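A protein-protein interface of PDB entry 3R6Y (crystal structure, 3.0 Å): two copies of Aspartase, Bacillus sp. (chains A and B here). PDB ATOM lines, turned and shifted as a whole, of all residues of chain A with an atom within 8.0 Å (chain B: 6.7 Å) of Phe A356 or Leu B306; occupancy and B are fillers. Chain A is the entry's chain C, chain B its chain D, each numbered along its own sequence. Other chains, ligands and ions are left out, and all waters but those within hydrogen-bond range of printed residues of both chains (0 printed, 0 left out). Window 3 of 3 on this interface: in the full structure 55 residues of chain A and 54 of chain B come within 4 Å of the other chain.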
ATOM      1  N   VAL A 232     -13.680  23.586  -7.242  1.00  0.00           N
ATOM      2  CA  VAL A 232     -12.270  23.597  -7.641  1.00  0.00           C
ATOM      3  C   VAL A 232     -12.026  24.492  -8.848  1.00  0.00           C
ATOM      4  O   VAL A 232     -11.269  25.456  -8.765  1.00  0.00           O
ATOM      5  CB  VAL A 232     -11.761  22.178  -7.964  1.00  0.00           C
ATOM      6  CG1 VAL A 232     -10.285  22.216  -8.332  1.00  0.00           C
ATOM      7  CG2 VAL A 232     -11.990  21.251  -6.782  1.00  0.00           C
ATOM      8  N   VAL A 265     -10.040  27.162 -12.969  1.00  0.00           N
ATOM      9  CA  VAL A 265      -9.156  26.817 -11.851  1.00  0.00           C
ATOM     10  C   VAL A 265      -8.386  28.069 -11.427  1.00  0.00           C
ATOM     11  O   VAL A 265      -8.376  28.428 -10.248  1.00  0.00           O
ATOM     12  CB  VAL A 265      -8.156  25.690 -12.210  1.00  0.00           C
ATOM     13  CG1 VAL A 265      -7.284  25.349 -11.014  1.00  0.00           C
ATOM     14  CG2 VAL A 265      -8.895  24.452 -12.701  1.00  0.00           C
ATOM     15  N   THR A 268     -10.176  30.545  -9.403  1.00  0.00           N
ATOM     16  CA  THR A 268     -10.655  30.052  -8.103  1.00  0.00           C
ATOM     17  C   THR A 268      -9.587  29.995  -6.998  1.00  0.00           C
ATOM     18  O   THR A 268      -9.923  30.102  -5.818  1.00  0.00           O
ATOM     19  CB  THR A 268     -11.305  28.652  -8.237  1.00  0.00           C
ATOM     20  OG1 THR A 268     -12.297  28.672  -9.272  1.00  0.00           O
ATOM     21  CG2 THR A 268     -11.963  28.236  -6.927  1.00  0.00           C
ATOM     22  N   GLN A 269      -8.317  29.825  -7.365  1.00  0.00           N
ATOM     23  CA  GLN A 269      -7.248  29.668  -6.373  1.00  0.00           C
ATOM     24  C   GLN A 269      -6.375  30.918  -6.238  1.00  0.00           C
ATOM     25  O   GLN A 269      -6.024  31.309  -5.123  1.00  0.00           O
ATOM     26  CB  GLN A 269      -6.396  28.432  -6.690  1.00  0.00           C
ATOM     27  CG  GLN A 269      -5.432  28.555  -7.855  1.00  0.00           C
ATOM     28  CD  GLN A 269      -4.667  27.273  -8.088  1.00  0.00           C
ATOM     29  OE1 GLN A 269      -5.253  26.247  -8.414  1.00  0.00           O
ATOM     30  NE2 GLN A 269      -3.351  27.321  -7.911  1.00  0.00           N
ATOM     31  N   ASN A 270      -6.024  31.533  -7.368  1.00  0.00           N
ATOM     32  CA  ASN A 270      -5.245  32.769  -7.370  1.00  0.00           C
ATOM     33  C   ASN A 270      -6.066  33.951  -6.835  1.00  0.00           C
ATOM     34  O   ASN A 270      -7.300  33.971  -6.921  1.00  0.00           O
ATOM     35  CB  ASN A 270      -4.734  33.081  -8.775  1.00  0.00           C
ATOM     36  CG  ASN A 270      -3.643  32.122  -9.235  1.00  0.00           C
ATOM     37  OD1 ASN A 270      -2.545  32.104  -8.690  1.00  0.00           O
ATOM     38  ND2 ASN A 270      -3.931  31.351 -10.273  1.00  0.00           N
ATOM     39  N   ALA A 353      -0.846  33.291   2.024  1.00  0.00           N
ATOM     40  CA  ALA A 353      -1.192  32.071   2.744  1.00  0.00           C
ATOM     41  C   ALA A 353      -1.932  31.046   1.900  1.00  0.00           C
ATOM     42  O   ALA A 353      -2.238  29.964   2.397  1.00  0.00           O
ATOM     43  CB  ALA A 353      -2.032  32.414   3.975  1.00  0.00           C
ATOM     44  N   GLY A 354      -2.235  31.382   0.646  1.00  0.00           N
ATOM     45  CA  GLY A 354      -2.989  30.499  -0.241  1.00  0.00           C
ATOM     46  C   GLY A 354      -2.400  29.103  -0.344  1.00  0.00           C
ATOM     47  O   GLY A 354      -1.175  28.927  -0.265  1.00  0.00           O
ATOM     48  N   GLN A 355      -3.276  28.113  -0.525  1.00  0.00           N
ATOM     49  CA  GLN A 355      -2.856  26.723  -0.654  1.00  0.00           C
ATOM     50  C   GLN A 355      -3.671  25.968  -1.692  1.00  0.00           C
ATOM     51  O   GLN A 355      -4.885  25.831  -1.567  1.00  0.00           O
ATOM     52  CB  GLN A 355      -2.945  26.019   0.695  1.00  0.00           C
ATOM     53  CG  GLN A 355      -1.748  26.294   1.588  1.00  0.00           C
ATOM     54  CD  GLN A 355      -1.972  25.904   3.024  1.00  0.00           C
ATOM     55  OE1 GLN A 355      -3.107  25.881   3.510  1.00  0.00           O
ATOM     56  NE2 GLN A 355      -0.884  25.609   3.723  1.00  0.00           N
ATOM     57  N   PHE A 356      -2.978  25.491  -2.721  1.00  0.00           N
ATOM     58  CA  PHE A 356      -3.556  24.622  -3.756  1.00  0.00           C
ATOM     59  C   PHE A 356      -4.718  25.253  -4.548  1.00  0.00           C
ATOM     60  O   PHE A 356      -4.483  26.199  -5.305  1.00  0.00           O
ATOM     61  CB  PHE A 356      -3.887  23.233  -3.179  1.00  0.00           C
ATOM     62  CG  PHE A 356      -2.664  22.376  -2.948  1.00  0.00           C
ATOM     63  CD1 PHE A 356      -1.749  22.167  -3.971  1.00  0.00           C
ATOM     64  CD2 PHE A 356      -2.423  21.791  -1.713  1.00  0.00           C
ATOM     65  CE1 PHE A 356      -0.629  21.398  -3.774  1.00  0.00           C
ATOM     66  CE2 PHE A 356      -1.295  21.018  -1.509  1.00  0.00           C
ATOM     67  CZ  PHE A 356      -0.396  20.823  -2.540  1.00  0.00           C
ATOM     68  N   GLU A 357      -5.947  24.754  -4.415  1.00  0.00           N
ATOM     69  CA  GLU A 357      -7.009  25.211  -5.301  1.00  0.00           C
ATOM     70  C   GLU A 357      -7.854  26.288  -4.631  1.00  0.00           C
ATOM     71  O   GLU A 357      -8.744  26.854  -5.272  1.00  0.00           O
ATOM     72  CB  GLU A 357      -7.910  24.069  -5.791  1.00  0.00           C
ATOM     73  CG  GLU A 357      -7.313  22.662  -5.846  1.00  0.00           C
ATOM     74  CD  GLU A 357      -5.910  22.568  -6.428  1.00  0.00           C
ATOM     75  OE1 GLU A 357      -5.627  23.166  -7.481  1.00  0.00           O
ATOM     76  OE2 GLU A 357      -5.084  21.855  -5.827  1.00  0.00           O
ATOM     77  N   LEU A 358      -7.589  26.589  -3.362  1.00  0.00           N
ATOM     78  CA  LEU A 358      -8.374  27.608  -2.660  1.00  0.00           C
ATOM     79  C   LEU A 358      -7.597  28.311  -1.541  1.00  0.00           C
ATOM     80  O   LEU A 358      -7.007  27.658  -0.665  1.00  0.00           O
ATOM     81  CB  LEU A 358      -9.648  26.991  -2.080  1.00  0.00           C
ATOM     82  CG  LEU A 358     -10.633  27.976  -1.451  1.00  0.00           C
ATOM     83  CD1 LEU A 358     -11.346  28.731  -2.547  1.00  0.00           C
ATOM     84  CD2 LEU A 358     -11.628  27.265  -0.534  1.00  0.00           C
ATOM     85  N   ASN A 359      -7.617  29.644  -1.586  1.00  0.00           N
ATOM     86  CA  ASN A 359      -7.076  30.478  -0.524  1.00  0.00           C
ATOM     87  C   ASN A 359      -8.152  30.695   0.531  1.00  0.00           C
ATOM     88  O   ASN A 359      -9.065  31.498   0.342  1.00  0.00           O
ATOM     89  CB  ASN A 359      -6.605  31.814  -1.098  1.00  0.00           C
ATOM     90  CG  ASN A 359      -5.917  32.690  -0.061  1.00  0.00           C
ATOM     91  OD1 ASN A 359      -6.453  32.927   1.028  1.00  0.00           O
ATOM     92  ND2 ASN A 359      -4.724  33.186  -0.402  1.00  0.00           N
ATOM     93  N   LYS B 183      -4.177  13.856  -9.809  1.00  0.00           N
ATOM     94  CA  LYS B 183      -3.909  14.009  -8.377  1.00  0.00           C
ATOM     95  C   LYS B 183      -5.142  14.564  -7.675  1.00  0.00           C
ATOM     96  O   LYS B 183      -6.126  14.927  -8.326  1.00  0.00           O
ATOM     97  CB  LYS B 183      -2.698  14.923  -8.124  1.00  0.00           C
ATOM     98  CG  LYS B 183      -2.765  16.281  -8.822  1.00  0.00           C
ATOM     99  CD  LYS B 183      -1.889  17.323  -8.137  1.00  0.00           C
ATOM    100  CE  LYS B 183      -2.577  17.902  -6.915  1.00  0.00           C
ATOM    101  NZ  LYS B 183      -1.822  19.044  -6.336  1.00  0.00           N
ATOM    102  N   MET B 184      -5.087  14.626  -6.346  1.00  0.00           N
ATOM    103  CA  MET B 184      -6.194  15.166  -5.565  1.00  0.00           C
ATOM    104  C   MET B 184      -6.112  16.682  -5.551  1.00  0.00           C
ATOM    105  O   MET B 184      -5.083  17.250  -5.199  1.00  0.00           O
ATOM    106  CB  MET B 184      -6.166  14.629  -4.132  1.00  0.00           C
ATOM    107  CG  MET B 184      -7.454  14.865  -3.346  1.00  0.00           C
ATOM    108  SD  MET B 184      -8.900  14.106  -4.119  1.00  0.00           S
ATOM    109  CE  MET B 184      -8.431  12.371  -4.112  1.00  0.00           C
ATOM    110  N   GLY B 185      -7.196  17.327  -5.967  1.00  0.00           N
ATOM    111  CA  GLY B 185      -7.327  18.774  -5.855  1.00  0.00           C
ATOM    112  C   GLY B 185      -7.772  19.051  -4.444  1.00  0.00           C
ATOM    113  O   GLY B 185      -8.624  18.327  -3.919  1.00  0.00           O
ATOM    114  N   ARG B 186      -7.180  20.061  -3.811  1.00  0.00           N
ATOM    115  CA  ARG B 186      -7.450  20.314  -2.403  1.00  0.00           C
ATOM    116  C   ARG B 186      -8.036  21.682  -2.122  1.00  0.00           C
ATOM    117  O   ARG B 186      -7.706  22.652  -2.785  1.00  0.00           O
ATOM    118  CB  ARG B 186      -6.177  20.114  -1.582  1.00  0.00           C
ATOM    119  CG  ARG B 186      -5.651  18.690  -1.638  1.00  0.00           C
ATOM    120  CD  ARG B 186      -4.542  18.441  -0.629  1.00  0.00           C
ATOM    121  NE  ARG B 186      -3.855  17.174  -0.869  1.00  0.00           N
ATOM    122  CZ  ARG B 186      -3.003  16.948  -1.868  1.00  0.00           C
ATOM    123  NH1 ARG B 186      -2.722  17.898  -2.753  1.00  0.00           N
ATOM    124  NH2 ARG B 186      -2.428  15.760  -1.994  1.00  0.00           N
ATOM    125  N   THR B 187      -8.915  21.735  -1.127  1.00  0.00           N
ATOM    126  CA  THR B 187      -9.434  22.986  -0.592  1.00  0.00           C
ATOM    127  C   THR B 187      -9.365  22.910   0.938  1.00  0.00           C
ATOM    128  O   THR B 187      -9.680  21.868   1.516  1.00  0.00           O
ATOM    129  CB  THR B 187     -10.884  23.222  -1.055  1.00  0.00           C
ATOM    130  OG1 THR B 187     -11.700  22.103  -0.688  1.00  0.00           O
ATOM    131  CG2 THR B 187     -10.936  23.405  -2.560  1.00  0.00           C
ATOM    132  N   LEU B 189      -6.782  22.587   2.589  1.00  0.00           N
ATOM    133  CA  LEU B 189      -5.868  21.447   2.793  1.00  0.00           C
ATOM    134  C   LEU B 189      -6.582  20.095   2.998  1.00  0.00           C
ATOM    135  O   LEU B 189      -6.009  19.165   3.573  1.00  0.00           O
ATOM    136  CB  LEU B 189      -4.903  21.716   3.956  1.00  0.00           C
ATOM    137  CG  LEU B 189      -3.564  22.355   3.598  1.00  0.00           C
ATOM    138  CD1 LEU B 189      -2.800  22.647   4.891  1.00  0.00           C
ATOM    139  CD2 LEU B 189      -2.752  21.462   2.646  1.00  0.00           C
ATOM    140  N   GLU B 200      -2.997  22.803 -12.482  1.00  0.00           N
ATOM    141  CA  GLU B 200      -2.333  23.650 -11.492  1.00  0.00           C
ATOM    142  C   GLU B 200      -1.224  24.463 -12.143  1.00  0.00           C
ATOM    143  O   GLU B 200      -1.248  25.685 -12.091  1.00  0.00           O
ATOM    144  CB  GLU B 200      -1.793  22.835 -10.321  1.00  0.00           C
ATOM    145  CG  GLU B 200      -2.880  22.437  -9.340  1.00  0.00           C
ATOM    146  CD  GLU B 200      -2.349  21.709  -8.133  1.00  0.00           C
ATOM    147  OE1 GLU B 200      -1.112  21.606  -7.978  1.00  0.00           O
ATOM    148  OE2 GLU B 200      -3.176  21.241  -7.336  1.00  0.00           O
ATOM    149  N   TYR B 204      -0.523  28.500 -12.394  1.00  0.00           N
ATOM    150  CA  TYR B 204       0.733  29.163 -12.045  1.00  0.00           C
ATOM    151  C   TYR B 204       1.248  29.963 -13.228  1.00  0.00           C
ATOM    152  O   TYR B 204       1.722  31.080 -13.055  1.00  0.00           O
ATOM    153  CB  TYR B 204       1.805  28.168 -11.568  1.00  0.00           C
ATOM    154  CG  TYR B 204       1.403  27.318 -10.371  1.00  0.00           C
ATOM    155  CD1 TYR B 204       0.375  27.717  -9.507  1.00  0.00           C
ATOM    156  CD2 TYR B 204       2.053  26.123 -10.097  1.00  0.00           C
ATOM    157  CE1 TYR B 204       0.007  26.942  -8.417  1.00  0.00           C
ATOM    158  CE2 TYR B 204       1.692  25.345  -9.007  1.00  0.00           C
ATOM    159  CZ  TYR B 204       0.667  25.760  -8.173  1.00  0.00           C
ATOM    160  OH  TYR B 204       0.286  25.000  -7.094  1.00  0.00           O
ATOM    161  N   LYS B 290       3.399  31.795  -3.043  1.00  0.00           N
ATOM    162  CA  LYS B 290       2.319  30.804  -3.018  1.00  0.00           C
ATOM    163  C   LYS B 290       2.733  29.622  -3.885  1.00  0.00           C
ATOM    164  O   LYS B 290       2.755  28.490  -3.420  1.00  0.00           O
ATOM    165  CB  LYS B 290       0.997  31.414  -3.519  1.00  0.00           C
ATOM    166  CG  LYS B 290      -0.281  30.667  -3.114  1.00  0.00           C
ATOM    167  CD  LYS B 290      -0.690  29.581  -4.127  1.00  0.00           C
ATOM    168  CE  LYS B 290      -1.931  28.793  -3.652  1.00  0.00           C
ATOM    169  NZ  LYS B 290      -2.406  27.793  -4.626  1.00  0.00           N
ATOM    170  N   ASN B 293       5.200  27.626  -1.948  1.00  0.00           N
ATOM    171  CA  ASN B 293       4.560  26.877  -0.861  1.00  0.00           C
ATOM    172  C   ASN B 293       3.794  25.643  -1.334  1.00  0.00           C
ATOM    173  O   ASN B 293       3.810  24.609  -0.666  1.00  0.00           O
ATOM    174  CB  ASN B 293       3.592  27.760  -0.078  1.00  0.00           C
ATOM    175  CG  ASN B 293       4.259  28.949   0.545  1.00  0.00           C
ATOM    176  OD1 ASN B 293       5.455  28.925   0.829  1.00  0.00           O
ATOM    177  ND2 ASN B 293       3.486  30.013   0.761  1.00  0.00           N
ATOM    178  N   ASP B 294       3.105  25.761  -2.465  1.00  0.00           N
ATOM    179  CA  ASP B 294       2.469  24.610  -3.091  1.00  0.00           C
ATOM    180  C   ASP B 294       3.527  23.587  -3.512  1.00  0.00           C
ATOM    181  O   ASP B 294       3.431  22.411  -3.163  1.00  0.00           O
ATOM    182  CB  ASP B 294       1.637  25.025  -4.318  1.00  0.00           C
ATOM    183  CG  ASP B 294       0.236  25.532  -3.956  1.00  0.00           C
ATOM    184  OD1 ASP B 294      -0.454  26.050  -4.867  1.00  0.00           O
ATOM    185  OD2 ASP B 294      -0.187  25.427  -2.781  1.00  0.00           O
ATOM    186  N   LEU B 295       4.533  24.036  -4.258  1.00  0.00           N
ATOM    187  CA  LEU B 295       5.561  23.134  -4.758  1.00  0.00           C
ATOM    188  C   LEU B 295       6.104  22.290  -3.625  1.00  0.00           C
ATOM    189  O   LEU B 295       6.044  21.068  -3.677  1.00  0.00           O
ATOM    190  CB  LEU B 295       6.698  23.900  -5.428  1.00  0.00           C
ATOM    191  CG  LEU B 295       6.343  24.494  -6.788  1.00  0.00           C
ATOM    192  CD1 LEU B 295       7.436  25.439  -7.248  1.00  0.00           C
ATOM    193  CD2 LEU B 295       6.108  23.383  -7.806  1.00  0.00           C
ATOM    194  N   LEU B 297       4.865  21.611  -0.720  1.00  0.00           N
ATOM    195  CA  LEU B 297       3.815  20.693  -0.257  1.00  0.00           C
ATOM    196  C   LEU B 297       3.680  19.492  -1.181  1.00  0.00           C
ATOM    197  O   LEU B 297       3.550  18.361  -0.725  1.00  0.00           O
ATOM    198  CB  LEU B 297       2.451  21.395  -0.177  1.00  0.00           C
ATOM    199  CG  LEU B 297       2.049  22.165   1.090  1.00  0.00           C
ATOM    200  CD1 LEU B 297       0.721  22.867   0.844  1.00  0.00           C
ATOM    201  CD2 LEU B 297       1.947  21.261   2.321  1.00  0.00           C
ATOM    202  N   MET B 298       3.686  19.754  -2.483  1.00  0.00           N
ATOM    203  CA  MET B 298       3.630  18.693  -3.489  1.00  0.00           C
ATOM    204  C   MET B 298       4.870  17.811  -3.391  1.00  0.00           C
ATOM    205  O   MET B 298       4.789  16.588  -3.509  1.00  0.00           O
ATOM    206  CB  MET B 298       3.513  19.290  -4.901  1.00  0.00           C
ATOM    207  CG  MET B 298       2.215  20.078  -5.134  1.00  0.00           C
ATOM    208  SD  MET B 298       1.921  20.607  -6.848  1.00  0.00           S
ATOM    209  CE  MET B 298       3.432  21.509  -7.191  1.00  0.00           C
ATOM    210  N   ALA B 299       6.013  18.437  -3.141  1.00  0.00           N
ATOM    211  CA  ALA B 299       7.285  17.732  -3.107  1.00  0.00           C
ATOM    212  C   ALA B 299       7.586  17.094  -1.762  1.00  0.00           C
ATOM    213  O   ALA B 299       8.699  16.624  -1.551  1.00  0.00           O
ATOM    214  CB  ALA B 299       8.422  18.682  -3.490  1.00  0.00           C
ATOM    215  N   SER B 300       6.622  17.071  -0.849  1.00  0.00           N
ATOM    216  CA  SER B 300       6.877  16.522   0.487  1.00  0.00           C
ATOM    217  C   SER B 300       6.984  14.997   0.437  1.00  0.00           C
ATOM    218  O   SER B 300       6.697  14.382  -0.595  1.00  0.00           O
ATOM    219  CB  SER B 300       5.801  16.972   1.488  1.00  0.00           C
ATOM    220  OG  SER B 300       4.499  16.886   0.927  1.00  0.00           O
ATOM    221  N   GLY B 301       7.430  14.409   1.546  1.00  0.00           N
ATOM    222  CA  GLY B 301       7.547  12.953   1.671  1.00  0.00           C
ATOM    223  C   GLY B 301       8.911  12.514   2.168  1.00  0.00           C
ATOM    224  O   GLY B 301       9.578  13.273   2.867  1.00  0.00           O
ATOM    225  N   PRO B 302       9.357  11.297   1.787  1.00  0.00           N
ATOM    226  CA  PRO B 302       8.716  10.332   0.867  1.00  0.00           C
ATOM    227  C   PRO B 302       7.510   9.556   1.414  1.00  0.00           C
ATOM    228  O   PRO B 302       6.586   9.265   0.656  1.00  0.00           O
ATOM    229  CB  PRO B 302       9.851   9.364   0.510  1.00  0.00           C
ATOM    230  CG  PRO B 302      10.876   9.539   1.553  1.00  0.00           C
ATOM    231  CD  PRO B 302      10.731  10.896   2.143  1.00  0.00           C
ATOM    232  N   ALA B 304       5.718  10.248   4.614  1.00  0.00           N
ATOM    233  CA  ALA B 304       4.794  11.007   5.470  1.00  0.00           C
ATOM    234  C   ALA B 304       4.431  12.364   4.842  1.00  0.00           C
ATOM    235  O   ALA B 304       4.255  13.373   5.540  1.00  0.00           O
ATOM    236  CB  ALA B 304       5.405  11.200   6.854  1.00  0.00           C
ATOM    237  N   GLY B 305       4.311  12.377   3.517  1.00  0.00           N
ATOM    238  CA  GLY B 305       4.068  13.608   2.773  1.00  0.00           C
ATOM    239  C   GLY B 305       3.011  13.423   1.711  1.00  0.00           C
ATOM    240  O   GLY B 305       2.173  12.526   1.804  1.00  0.00           O
ATOM    241  N   LEU B 306       3.043  14.287   0.703  1.00  0.00           N
ATOM    242  CA  LEU B 306       2.095  14.213  -0.399  1.00  0.00           C
ATOM    243  C   LEU B 306       2.726  13.548  -1.624  1.00  0.00           C
ATOM    244  O   LEU B 306       2.028  12.912  -2.401  1.00  0.00           O
ATOM    245  CB  LEU B 306       1.561  15.605  -0.729  1.00  0.00           C
ATOM    246  CG  LEU B 306       0.504  16.164   0.237  1.00  0.00           C
ATOM    247  CD1 LEU B 306       0.913  16.012   1.691  1.00  0.00           C
ATOM    248  CD2 LEU B 306       0.210  17.619  -0.075  1.00  0.00           C
ATOM    249  N   SER B 307       4.041  13.694  -1.779  1.00  0.00           N
ATOM    250  CA  SER B 307       4.806  13.012  -2.827  1.00  0.00           C
ATOM    251  C   SER B 307       4.127  13.079  -4.194  1.00  0.00           C
ATOM    252  O   SER B 307       3.948  12.058  -4.861  1.00  0.00           O
ATOM    253  CB  SER B 307       5.079  11.561  -2.425  1.00  0.00           C
ATOM    254  OG  SER B 307       6.104  11.498  -1.452  1.00  0.00           O
ATOM    255  N   GLU B 308       3.747  14.291  -4.599  1.00  0.00           N
ATOM    256  CA  GLU B 308       3.082  14.512  -5.887  1.00  0.00           C
ATOM    257  C   GLU B 308       4.075  14.867  -6.980  1.00  0.00           C
ATOM    258  O   GLU B 308       3.806  14.638  -8.160  1.00  0.00           O
ATOM    259  CB  GLU B 308       2.042  15.622  -5.779  1.00  0.00           C
ATOM    260  CG  GLU B 308       0.826  15.229  -4.964  1.00  0.00           C
ATOM    261  CD  GLU B 308      -0.217  16.332  -4.888  1.00  0.00           C
ATOM    262  OE1 GLU B 308      -1.286  16.089  -4.287  1.00  0.00           O
ATOM    263  OE2 GLU B 308       0.030  17.437  -5.422  1.00  0.00           O
ATOM    264  N   ILE B 309       5.211  15.442  -6.589  1.00  0.00           N
ATOM    265  CA  ILE B 309       6.270  15.798  -7.527  1.00  0.00           C
ATOM    266  C   ILE B 309       7.638  15.491  -6.922  1.00  0.00           C
ATOM    267  O   ILE B 309       7.762  15.320  -5.706  1.00  0.00           O
ATOM    268  CB  ILE B 309       6.195  17.287  -7.920  1.00  0.00           C
ATOM    269  CG1 ILE B 309       6.392  18.186  -6.690  1.00  0.00           C
ATOM    270  CG2 ILE B 309       4.862  17.577  -8.583  1.00  0.00           C
ATOM    271  CD1 ILE B 309       6.351  19.671  -6.984  1.00  0.00           C
ATOM    272  N   ASN B 394       5.130  12.241  -9.817  1.00  0.00           N
ATOM    273  CA  ASN B 394       5.274  11.003  -9.052  1.00  0.00           C
ATOM    274  C   ASN B 394       4.220   9.994  -9.498  1.00  0.00           C
ATOM    275  O   ASN B 394       3.197  10.371 -10.073  1.00  0.00           O
ATOM    276  CB  ASN B 394       5.130  11.290  -7.550  1.00  0.00           C
ATOM    277  CG  ASN B 394       6.046  10.423  -6.688  1.00  0.00           C
ATOM    278  OD1 ASN B 394       6.230   9.235  -6.950  1.00  0.00           O
ATOM    279  ND2 ASN B 394       6.621  11.023  -5.646  1.00  0.00           N
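The side-chain amino group (NZ) of Lys B290 lies close to the side-chain amide nitrogen (NE2) of Gln A269 (3.5 Å).
The side-chain amino group (NZ) of Lys B290 sits at hydrogen-bond distance from the backbone carbonyl oxygen (O) of Phe A356 (2.7 Å).
N of Phe A356 is in hydrogen-bond range of OD2 of Asp B294.
O of Arg B186 sits close to N of Glu A357 (3.2 Å).
OE2 of Glu B200 lies close to OE2 of Glu A357 (2.5 Å).
NE2 of Gln A269 sits close to O of Phe A356, at 3.1 Å.
The side-chain amino group (NZ) of Lys B183 is in salt-bridge range of the side-chain carboxylate (OE2) of Glu B200, 2.8 Å away.
The backbone carbonyl oxygen of Met B184 is in hydrogen-bond range of the guanidinium group of Arg B186 (3.5 Å).
NH2 of Arg B186 is in salt-bridge range of OE1 of Glu B308 (2.6 Å).
The side-chain hydroxyl (OG) of Ser B300 is in hydrogen-bond range of the backbone carbonyl oxygen (O) of Leu B297 (2.4 Å).
The backbone carbonyl oxygen (O) of Met B298 sits at hydrogen-bond distance from the backbone NH (N) of Glu B308, at 2.7 Å.
Among the printed residues, merely in contact across the chains: Gln A269 with Tyr B204, Gly A354 with Lys B290, Gln A355 with Leu B189, Gln A355 with Lys B290, Gln A355 with Asp B294, Phe A356 with Lys B183, Phe A356 with Arg B186, Phe A356 with Glu B200, Phe A356 with Leu B297, Phe A356 with Met B298, Phe A356 with Leu B306, Glu A357 with Gly B185, Leu A358 with Arg B186 and Leu A358 with Thr B187.
Printed residues of chain B within 4 Å of Gln A269: Tyr B204 and Lys B290.
Of the printed residues of chain B, Phe A356 touches Lys B183, Arg B186, Glu B200, Lys B290, Asp B294, Leu B297, Met B298 and Leu B306.
Of the printed residues of chain A, Leu B297 touches Phe A356 (3.6 Å).
No residue of chain A comes within 4 Å of Gly B305.
Printed residues of chain A within 4 Å of Leu B306: Phe A356 (3.98 Å).
The nearest printed residue of chain B that does not touch Phe A356 is Glu B308 (4.3 Å).
Hydrophobic or aromatic side chains of chain B that line the printed part of chain A: Leu B189, Tyr B204, Leu B297, Met B298 and Leu B306.
Of the 12 printed residues of chain A, 6 touch a printed residue of chain B.
Hydrophobic or aromatic side chains of chain A that line the printed part of chain B: Phe A356 and Leu A358.
Among the printed residues, 19 pairs touch across the chains.
Among the printed residues, no Asp or Glu carboxylate lies within 4 Å of a Lys or Arg side-chain nitrogen of the other chain.
No position is printed for both chains.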
